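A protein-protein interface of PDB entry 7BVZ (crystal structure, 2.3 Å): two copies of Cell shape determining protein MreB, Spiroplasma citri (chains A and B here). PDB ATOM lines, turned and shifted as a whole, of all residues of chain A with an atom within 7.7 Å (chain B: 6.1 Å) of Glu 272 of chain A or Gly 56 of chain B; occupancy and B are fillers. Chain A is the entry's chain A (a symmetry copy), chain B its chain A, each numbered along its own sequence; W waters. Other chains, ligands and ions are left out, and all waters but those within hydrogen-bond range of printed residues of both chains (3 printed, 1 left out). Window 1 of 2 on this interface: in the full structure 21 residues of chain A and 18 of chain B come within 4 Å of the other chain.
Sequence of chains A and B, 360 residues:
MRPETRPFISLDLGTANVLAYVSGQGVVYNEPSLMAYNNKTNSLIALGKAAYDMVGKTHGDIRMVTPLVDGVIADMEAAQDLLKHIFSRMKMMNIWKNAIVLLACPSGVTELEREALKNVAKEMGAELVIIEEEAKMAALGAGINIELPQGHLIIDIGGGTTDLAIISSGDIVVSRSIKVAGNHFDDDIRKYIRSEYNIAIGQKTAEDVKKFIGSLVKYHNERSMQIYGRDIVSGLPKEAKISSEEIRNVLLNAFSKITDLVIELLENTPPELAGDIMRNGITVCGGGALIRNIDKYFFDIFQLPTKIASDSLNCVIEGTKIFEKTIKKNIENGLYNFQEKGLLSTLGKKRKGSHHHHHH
OE2 of Glu 272 of chain A lies close to N of Lys 204 of chain B (3.4 Å).
The side-chain amino group (NZ) of Lys 57 of chain B is in salt-bridge range of the side-chain carboxylate (OD2) of Asp 276 of chain A (3.1 Å).
O of Pro 149 of chain A is in hydrogen-bond range of NZ of Lys 57 of chain B (2.9 Å).
OE1 of Glu 272 of chain A lies within hydrogen-bond range of OG1 of Thr 205 of chain B (2.8 Å).
N of Gly 151 of chain A is in hydrogen-bond range of OD2 of Asp 276 of chain A.
O of Gly 275 of chain A lies within hydrogen-bond range of NH1 of Arg 279 of chain A (3.4 Å).
OD1 of Asp 276 of chain A is in salt-bridge range of NH2 of Arg 279 of chain A.
NZ of Lys 57 of chain B touches NE2 of Gln 150 of chain A, 3.5 Å away.
Gly 56 of chain B touches Pro 270 of chain A.
CB of Pro 271 of chain A touches O of Ala 200 of chain B (3.2 Å).
Gly 56 of chain B touches Glu 272 of chain A (O to CB, 3.4 Å).
Lys 57 of chain B touches Glu 272 of chain A.
Gly 202 of chain B touches Glu 272 of chain A.
CD2 of Leu 273 of chain A touches O of Gly 56 of chain B, 3.2 Å away.
Leu 273 of chain A touches Lys 57 of chain B.
O of Gly 229 of chain B touches CB of Ala 274 of chain A (3.9 Å).
Gly 275 of chain A touches Tyr 228 of chain B.
Glu 272 of chain A touches just these residues of chain B: Gly 56 (3.4 Å), Lys 57 (3.6 Å), Gly 202 (3.4 Å), Lys 204 (3.4 Å) and Thr 205 (2.8 Å).
Of the printed residues of chain B, Leu 273 of chain A touches Gly 56 and Lys 57.
Of the printed residues of chain B, Gly 275 of chain A touches Tyr 228 (3.2 Å).
Gly 56 of chain B touches just these residues of chain A: Pro 270, Glu 272 and Leu 273.
Met 64 of chain B touches none of the printed residues of chain A.
Printed residues of chain A within 4 Å of Thr 205 of chain B: Glu 272.
Of the 15 printed residues of chain B, 9 touch a printed residue of chain A.
Hydrophobic or aromatic side chains of chain B that line the printed part of chain A: Tyr 228.
Hydrophobic or aromatic side chains of chain A that line the printed part of chain B: Pro 270, Pro 271, Leu 273 and Ala 274.
Along chain A the printed residues that touch a printed residue of chain B span positions 149 to 279.
Among the printed residues, 19 pairs touch across the chains.
Among the printed residues, Asp or Glu carboxylates within 4 Å of a Lys or Arg side-chain nitrogen of the other chain: Asp 276 of chain A with Lys 57 of chain B.
No position is printed for both chains.
Water W3 lies within hydrogen-bond range of the backbone carbonyl oxygen (O) of Lys 57 of chain B (2.4 Å) and the backbone carbonyl oxygen (O) of Ser 168 of chain A (3.0 Å).
Water W2 lies within hydrogen-bond range of the side-chain amino group of Lys 57 of chain B (2.7 Å), the side-chain carboxylate of Asp 276 of chain A (2.8 Å) and the guanidinium group of Arg 279 of chain A (3.3 Å).
Water W1 lies within hydrogen-bond range of the backbone carbonyl oxygen of Gly 56 of chain B (2.7 Å) and the backbone NH of Glu 272 of chain A (3.2 Å).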
ATOM      1  N   PRO A 149       0.236   1.987  -4.647  1.00  0.00           N
ATOM      2  CA  PRO A 149      -0.917   1.363  -3.975  1.00  0.00           C
ATOM      3  C   PRO A 149      -2.118   2.300  -3.890  1.00  0.00           C
ATOM      4  O   PRO A 149      -2.582   2.675  -2.809  1.00  0.00           O
ATOM      5  CB  PRO A 149      -0.339   1.015  -2.597  1.00  0.00           C
ATOM      6  CG  PRO A 149       0.687   2.064  -2.359  1.00  0.00           C
ATOM      7  CD  PRO A 149       1.303   2.351  -3.699  1.00  0.00           C
ATOM      8  N   GLN A 150      -2.631   2.694  -5.054  1.00  0.00           N
ATOM      9  CA  GLN A 150      -3.807   3.545  -5.158  1.00  0.00           C
ATOM     10  C   GLN A 150      -4.750   2.954  -6.193  1.00  0.00           C
ATOM     11  O   GLN A 150      -4.335   2.665  -7.319  1.00  0.00           O
ATOM     12  CB  GLN A 150      -3.429   4.980  -5.537  1.00  0.00           C
ATOM     13  CG  GLN A 150      -2.865   5.790  -4.383  1.00  0.00           C
ATOM     14  CD  GLN A 150      -3.881   6.011  -3.277  1.00  0.00           C
ATOM     15  OE1 GLN A 150      -5.063   6.238  -3.538  1.00  0.00           O
ATOM     16  NE2 GLN A 150      -3.423   5.942  -2.033  1.00  0.00           N
ATOM     17  N   GLY A 151      -6.012   2.777  -5.809  1.00  0.00           N
ATOM     18  CA  GLY A 151      -6.972   2.137  -6.691  1.00  0.00           C
ATOM     19  C   GLY A 151      -7.436   3.065  -7.804  1.00  0.00           C
ATOM     20  O   GLY A 151      -7.689   4.251  -7.594  1.00  0.00           O
ATOM     21  N   SER A 168      -4.616  -1.723  -8.686  1.00  0.00           N
ATOM     22  CA  SER A 168      -3.885  -1.175  -7.550  1.00  0.00           C
ATOM     23  C   SER A 168      -2.605  -1.977  -7.378  1.00  0.00           C
ATOM     24  O   SER A 168      -2.636  -3.210  -7.442  1.00  0.00           O
ATOM     25  CB  SER A 168      -4.727  -1.220  -6.270  1.00  0.00           C
ATOM     26  OG  SER A 168      -3.994  -0.738  -5.157  1.00  0.00           O
ATOM     27  N   VAL A 173      -7.298  -6.162  -9.170  1.00  0.00           N
ATOM     28  CA  VAL A 173      -7.992  -6.598  -7.961  1.00  0.00           C
ATOM     29  C   VAL A 173      -9.356  -7.179  -8.314  1.00  0.00           C
ATOM     30  O   VAL A 173      -9.677  -8.318  -7.958  1.00  0.00           O
ATOM     31  CB  VAL A 173      -8.116  -5.435  -6.961  1.00  0.00           C
ATOM     32  CG1 VAL A 173      -8.776  -5.909  -5.675  1.00  0.00           C
ATOM     33  CG2 VAL A 173      -6.748  -4.835  -6.676  1.00  0.00           C
ATOM     34  N   THR A 269     -15.973  -4.766  -4.801  1.00  0.00           N
ATOM     35  CA  THR A 269     -14.705  -4.066  -4.636  1.00  0.00           C
ATOM     36  C   THR A 269     -14.397  -3.901  -3.151  1.00  0.00           C
ATOM     37  O   THR A 269     -15.271  -3.464  -2.393  1.00  0.00           O
ATOM     38  CB  THR A 269     -14.755  -2.703  -5.315  1.00  0.00           C
ATOM     39  OG1 THR A 269     -14.989  -2.879  -6.718  1.00  0.00           O
ATOM     40  CG2 THR A 269     -13.453  -1.955  -5.122  1.00  0.00           C
ATOM     41  N   PRO A 270     -13.193  -4.253  -2.702  1.00  0.00           N
ATOM     42  CA  PRO A 270     -12.887  -4.144  -1.278  1.00  0.00           C
ATOM     43  C   PRO A 270     -13.070  -2.721  -0.796  1.00  0.00           C
ATOM     44  O   PRO A 270     -12.839  -1.755  -1.547  1.00  0.00           O
ATOM     45  CB  PRO A 270     -11.419  -4.586  -1.200  1.00  0.00           C
ATOM     46  CG  PRO A 270     -11.247  -5.493  -2.372  1.00  0.00           C
ATOM     47  CD  PRO A 270     -12.106  -4.903  -3.455  1.00  0.00           C
ATOM     48  N   PRO A 271     -13.488  -2.541   0.461  1.00  0.00           N
ATOM     49  CA  PRO A 271     -13.866  -1.193   0.923  1.00  0.00           C
ATOM     50  C   PRO A 271     -12.735  -0.183   0.865  1.00  0.00           C
ATOM     51  O   PRO A 271     -12.996   1.008   0.653  1.00  0.00           O
ATOM     52  CB  PRO A 271     -14.333  -1.437   2.366  1.00  0.00           C
ATOM     53  CG  PRO A 271     -13.677  -2.720   2.769  1.00  0.00           C
ATOM     54  CD  PRO A 271     -13.620  -3.551   1.524  1.00  0.00           C
ATOM     55  N   GLU A 272     -11.485  -0.617   1.042  1.00  0.00           N
ATOM     56  CA  GLU A 272     -10.371   0.320   0.957  1.00  0.00           C
ATOM     57  C   GLU A 272     -10.146   0.791  -0.475  1.00  0.00           C
ATOM     58  O   GLU A 272      -9.738   1.937  -0.689  1.00  0.00           O
ATOM     59  CB  GLU A 272      -9.102  -0.319   1.522  1.00  0.00           C
ATOM     60  CG  GLU A 272      -8.004   0.671   1.889  1.00  0.00           C
ATOM     61  CD  GLU A 272      -8.415   1.633   2.991  1.00  0.00           C
ATOM     62  OE1 GLU A 272      -8.615   2.830   2.698  1.00  0.00           O
ATOM     63  OE2 GLU A 272      -8.540   1.191   4.151  1.00  0.00           O
ATOM     64  N   LEU A 273     -10.405  -0.073  -1.463  1.00  0.00           N
ATOM     65  CA  LEU A 273     -10.313   0.349  -2.859  1.00  0.00           C
ATOM     66  C   LEU A 273     -11.416   1.337  -3.204  1.00  0.00           C
ATOM     67  O   LEU A 273     -11.165   2.365  -3.846  1.00  0.00           O
ATOM     68  CB  LEU A 273     -10.387  -0.858  -3.794  1.00  0.00           C
ATOM     69  CG  LEU A 273      -9.141  -1.688  -4.101  1.00  0.00           C
ATOM     70  CD1 LEU A 273      -7.915  -0.805  -4.297  1.00  0.00           C
ATOM     71  CD2 LEU A 273      -8.918  -2.713  -3.020  1.00  0.00           C
ATOM     72  N   ALA A 274     -12.653   1.032  -2.796  1.00  0.00           N
ATOM     73  CA  ALA A 274     -13.780   1.915  -3.082  1.00  0.00           C
ATOM     74  C   ALA A 274     -13.525   3.329  -2.583  1.00  0.00           C
ATOM     75  O   ALA A 274     -13.986   4.299  -3.195  1.00  0.00           O
ATOM     76  CB  ALA A 274     -15.057   1.353  -2.454  1.00  0.00           C
ATOM     77  N   GLY A 275     -12.785   3.468  -1.483  1.00  0.00           N
ATOM     78  CA  GLY A 275     -12.408   4.794  -1.025  1.00  0.00           C
ATOM     79  C   GLY A 275     -11.520   5.522  -2.015  1.00  0.00           C
ATOM     80  O   GLY A 275     -11.648   6.734  -2.204  1.00  0.00           O
ATOM     81  N   ASP A 276     -10.608   4.793  -2.663  1.00  0.00           N
ATOM     82  CA  ASP A 276      -9.737   5.419  -3.651  1.00  0.00           C
ATOM     83  C   ASP A 276     -10.494   5.768  -4.926  1.00  0.00           C
ATOM     84  O   ASP A 276     -10.113   6.709  -5.631  1.00  0.00           O
ATOM     85  CB  ASP A 276      -8.555   4.504  -3.973  1.00  0.00           C
ATOM     86  CG  ASP A 276      -7.710   4.190  -2.752  1.00  0.00           C
ATOM     87  OD1 ASP A 276      -7.891   4.853  -1.708  1.00  0.00           O
ATOM     88  OD2 ASP A 276      -6.858   3.282  -2.839  1.00  0.00           O
ATOM     89  N   ILE A 277     -11.562   5.029  -5.236  1.00  0.00           N
ATOM     90  CA  ILE A 277     -12.323   5.306  -6.450  1.00  0.00           C
ATOM     91  C   ILE A 277     -13.001   6.666  -6.362  1.00  0.00           C
ATOM     92  O   ILE A 277     -13.138   7.365  -7.373  1.00  0.00           O
ATOM     93  CB  ILE A 277     -13.342   4.180  -6.712  1.00  0.00           C
ATOM     94  CG1 ILE A 277     -12.655   2.813  -6.672  1.00  0.00           C
ATOM     95  CG2 ILE A 277     -14.025   4.381  -8.054  1.00  0.00           C
ATOM     96  CD1 ILE A 277     -11.565   2.637  -7.709  1.00  0.00           C
ATOM     97  N   ARG A 279     -11.786   9.310  -4.852  1.00  0.00           N
ATOM     98  CA  ARG A 279     -10.781  10.360  -4.965  1.00  0.00           C
ATOM     99  C   ARG A 279     -10.010  10.292  -6.278  1.00  0.00           C
ATOM    100  O   ARG A 279      -9.736  11.331  -6.886  1.00  0.00           O
ATOM    101  CB  ARG A 279      -9.809  10.288  -3.785  1.00  0.00           C
ATOM    102  CG  ARG A 279     -10.482  10.359  -2.423  1.00  0.00           C
ATOM    103  CD  ARG A 279      -9.459  10.494  -1.306  1.00  0.00           C
ATOM    104  NE  ARG A 279      -8.489   9.402  -1.314  1.00  0.00           N
ATOM    105  CZ  ARG A 279      -8.602   8.296  -0.586  1.00  0.00           C
ATOM    106  NH1 ARG A 279      -9.645   8.129   0.216  1.00  0.00           N
ATOM    107  NH2 ARG A 279      -7.671   7.355  -0.658  1.00  0.00           N
ATOM    108  N   MET B  54      -0.560  -1.697   1.188  1.00  0.00           N
ATOM    109  CA  MET B  54      -1.403  -2.529   0.345  1.00  0.00           C
ATOM    110  C   MET B  54      -2.490  -3.274   1.108  1.00  0.00           C
ATOM    111  O   MET B  54      -3.322  -3.928   0.470  1.00  0.00           O
ATOM    112  CB  MET B  54      -0.546  -3.549  -0.420  1.00  0.00           C
ATOM    113  CG  MET B  54       0.557  -2.938  -1.264  1.00  0.00           C
ATOM    114  SD  MET B  54       1.646  -4.193  -1.965  1.00  0.00           S
ATOM    115  CE  MET B  54       0.489  -5.155  -2.933  1.00  0.00           C
ATOM    116  N   VAL B  55      -2.504  -3.205   2.442  1.00  0.00           N
ATOM    117  CA  VAL B  55      -3.496  -3.949   3.210  1.00  0.00           C
ATOM    118  C   VAL B  55      -4.890  -3.453   2.855  1.00  0.00           C
ATOM    119  O   VAL B  55      -5.166  -2.247   2.867  1.00  0.00           O
ATOM    120  CB  VAL B  55      -3.209  -3.838   4.716  1.00  0.00           C
ATOM    121  CG1 VAL B  55      -3.060  -2.388   5.140  1.00  0.00           C
ATOM    122  CG2 VAL B  55      -4.307  -4.522   5.519  1.00  0.00           C
ATOM    123  N   GLY B  56      -5.775  -4.389   2.519  1.00  0.00           N
ATOM    124  CA  GLY B  56      -7.081  -4.037   2.006  1.00  0.00           C
ATOM    125  C   GLY B  56      -7.100  -3.636   0.550  1.00  0.00           C
ATOM    126  O   GLY B  56      -8.156  -3.229   0.052  1.00  0.00           O
ATOM    127  N   LYS B  57      -5.966  -3.739  -0.151  1.00  0.00           N
ATOM    128  CA  LYS B  57      -5.856  -3.334  -1.547  1.00  0.00           C
ATOM    129  C   LYS B  57      -5.215  -4.425  -2.396  1.00  0.00           C
ATOM    130  O   LYS B  57      -4.512  -4.129  -3.365  1.00  0.00           O
ATOM    131  CB  LYS B  57      -5.061  -2.035  -1.682  1.00  0.00           C
ATOM    132  CG  LYS B  57      -5.648  -0.845  -0.943  1.00  0.00           C
ATOM    133  CD  LYS B  57      -4.834   0.408  -1.217  1.00  0.00           C
ATOM    134  CE  LYS B  57      -5.381   1.606  -0.463  1.00  0.00           C
ATOM    135  NZ  LYS B  57      -4.625   2.850  -0.775  1.00  0.00           N
ATOM    136  N   THR B  58      -5.446  -5.691  -2.054  1.00  0.00           N
ATOM    137  CA  THR B  58      -4.764  -6.799  -2.705  1.00  0.00           C
ATOM    138  C   THR B  58      -5.761  -7.838  -3.193  1.00  0.00           C
ATOM    139  O   THR B  58      -6.831  -8.027  -2.608  1.00  0.00           O
ATOM    140  CB  THR B  58      -3.755  -7.471  -1.762  1.00  0.00           C
ATOM    141  OG1 THR B  58      -4.409  -7.841  -0.542  1.00  0.00           O
ATOM    142  CG2 THR B  58      -2.603  -6.531  -1.454  1.00  0.00           C
ATOM    143  N   MET B  64      -1.521 -11.372   3.228  1.00  0.00           N
ATOM    144  CA  MET B  64      -0.954 -10.461   4.213  1.00  0.00           C
ATOM    145  C   MET B  64      -0.669 -11.223   5.499  1.00  0.00           C
ATOM    146  O   MET B  64      -1.559 -11.881   6.048  1.00  0.00           O
ATOM    147  CB  MET B  64      -1.901  -9.292   4.485  1.00  0.00           C
ATOM    148  CG  MET B  64      -2.014  -8.318   3.328  1.00  0.00           C
ATOM    149  SD  MET B  64      -0.393  -7.867   2.684  1.00  0.00           S
ATOM    150  CE  MET B  64      -0.813  -6.442   1.692  1.00  0.00           C
ATOM    151  N   ALA B 200     -18.932   0.531   4.721  1.00  0.00           N
ATOM    152  CA  ALA B 200     -17.830  -0.369   5.025  1.00  0.00           C
ATOM    153  C   ALA B 200     -16.512   0.303   4.664  1.00  0.00           C
ATOM    154  O   ALA B 200     -16.338   0.779   3.537  1.00  0.00           O
ATOM    155  CB  ALA B 200     -17.980  -1.688   4.266  1.00  0.00           C
ATOM    156  N   ILE B 201     -15.592   0.351   5.625  1.00  0.00           N
ATOM    157  CA  ILE B 201     -14.273   0.926   5.413  1.00  0.00           C
ATOM    158  C   ILE B 201     -13.223  -0.133   5.721  1.00  0.00           C
ATOM    159  O   ILE B 201     -13.471  -1.101   6.444  1.00  0.00           O
ATOM    160  CB  ILE B 201     -14.036   2.188   6.269  1.00  0.00           C
ATOM    161  CG1 ILE B 201     -14.036   1.835   7.758  1.00  0.00           C
ATOM    162  CG2 ILE B 201     -15.087   3.242   5.966  1.00  0.00           C
ATOM    163  CD1 ILE B 201     -13.634   2.984   8.660  1.00  0.00           C
ATOM    164  N   GLY B 202     -12.035   0.063   5.152  1.00  0.00           N
ATOM    165  CA  GLY B 202     -10.930  -0.834   5.409  1.00  0.00           C
ATOM    166  C   GLY B 202     -10.258  -0.555   6.740  1.00  0.00           C
ATOM    167  O   GLY B 202     -10.561   0.414   7.436  1.00  0.00           O
ATOM    168  N   GLN B 203      -9.320  -1.438   7.094  1.00  0.00           N
ATOM    169  CA  GLN B 203      -8.597  -1.279   8.351  1.00  0.00           C
ATOM    170  C   GLN B 203      -7.693  -0.053   8.330  1.00  0.00           C
ATOM    171  O   GLN B 203      -7.461   0.561   9.378  1.00  0.00           O
ATOM    172  CB  GLN B 203      -7.778  -2.535   8.651  1.00  0.00           C
ATOM    173  CG  GLN B 203      -8.596  -3.816   8.727  1.00  0.00           C
ATOM    174  CD  GLN B 203      -9.500  -3.866   9.944  1.00  0.00           C
ATOM    175  OE1 GLN B 203     -10.601  -4.415   9.890  1.00  0.00           O
ATOM    176  NE2 GLN B 203      -9.035  -3.300  11.051  1.00  0.00           N
ATOM    177  N   LYS B 204      -7.177   0.320   7.155  1.00  0.00           N
ATOM    178  CA  LYS B 204      -6.267   1.457   7.077  1.00  0.00           C
ATOM    179  C   LYS B 204      -6.994   2.771   7.340  1.00  0.00           C
ATOM    180  O   LYS B 204      -6.480   3.637   8.058  1.00  0.00           O
ATOM    181  CB  LYS B 204      -5.581   1.488   5.711  1.00  0.00           C
ATOM    182  N   THR B 205      -8.185   2.939   6.763  1.00  0.00           N
ATOM    183  CA  THR B 205      -8.967   4.144   7.021  1.00  0.00           C
ATOM    184  C   THR B 205      -9.378   4.226   8.484  1.00  0.00           C
ATOM    185  O   THR B 205      -9.342   5.306   9.087  1.00  0.00           O
ATOM    186  CB  THR B 205     -10.198   4.174   6.115  1.00  0.00           C
ATOM    187  OG1 THR B 205      -9.783   4.269   4.745  1.00  0.00           O
ATOM    188  CG2 THR B 205     -11.092   5.360   6.456  1.00  0.00           C
ATOM    189  N   ALA B 206      -9.760   3.092   9.077  1.00  0.00           N
ATOM    190  CA  ALA B 206     -10.137   3.084  10.486  1.00  0.00           C
ATOM    191  C   ALA B 206      -8.961   3.470  11.377  1.00  0.00           C
ATOM    192  O   ALA B 206      -9.144   4.131  12.405  1.00  0.00           O
ATOM    193  CB  ALA B 206     -10.678   1.707  10.875  1.00  0.00           C
ATOM    194  N   TYR B 228     -13.935   7.461   3.248  1.00  0.00           N
ATOM    195  CA  TYR B 228     -14.330   7.007   1.917  1.00  0.00           C
ATOM    196  C   TYR B 228     -14.341   5.485   1.935  1.00  0.00           C
ATOM    197  O   TYR B 228     -13.288   4.856   2.080  1.00  0.00           O
ATOM    198  CB  TYR B 228     -13.380   7.537   0.841  1.00  0.00           C
ATOM    199  CG  TYR B 228     -13.151   9.033   0.877  1.00  0.00           C
ATOM    200  CD1 TYR B 228     -12.138   9.582   1.656  1.00  0.00           C
ATOM    201  CD2 TYR B 228     -13.937   9.895   0.124  1.00  0.00           C
ATOM    202  CE1 TYR B 228     -11.921  10.947   1.689  1.00  0.00           C
ATOM    203  CE2 TYR B 228     -13.727  11.263   0.151  1.00  0.00           C
ATOM    204  CZ  TYR B 228     -12.718  11.783   0.936  1.00  0.00           C
ATOM    205  OH  TYR B 228     -12.503  13.140   0.966  1.00  0.00           O
ATOM    206  N   GLY B 229     -15.527   4.897   1.797  1.00  0.00           N
ATOM    207  CA  GLY B 229     -15.659   3.454   1.813  1.00  0.00           C
ATOM    208  C   GLY B 229     -16.722   2.942   0.865  1.00  0.00           C
ATOM    209  O   GLY B 229     -17.102   3.638  -0.080  1.00  0.00           O
HETATM  210  O   HOH W   1     -10.316  -3.480   1.726  1.00  0.00           O
HETATM  211  O   HOH W   2      -6.183   4.617   0.473  1.00  0.00           O
HETATM  212  O   HOH W   3      -2.973  -4.917  -5.053  1.00  0.00           O
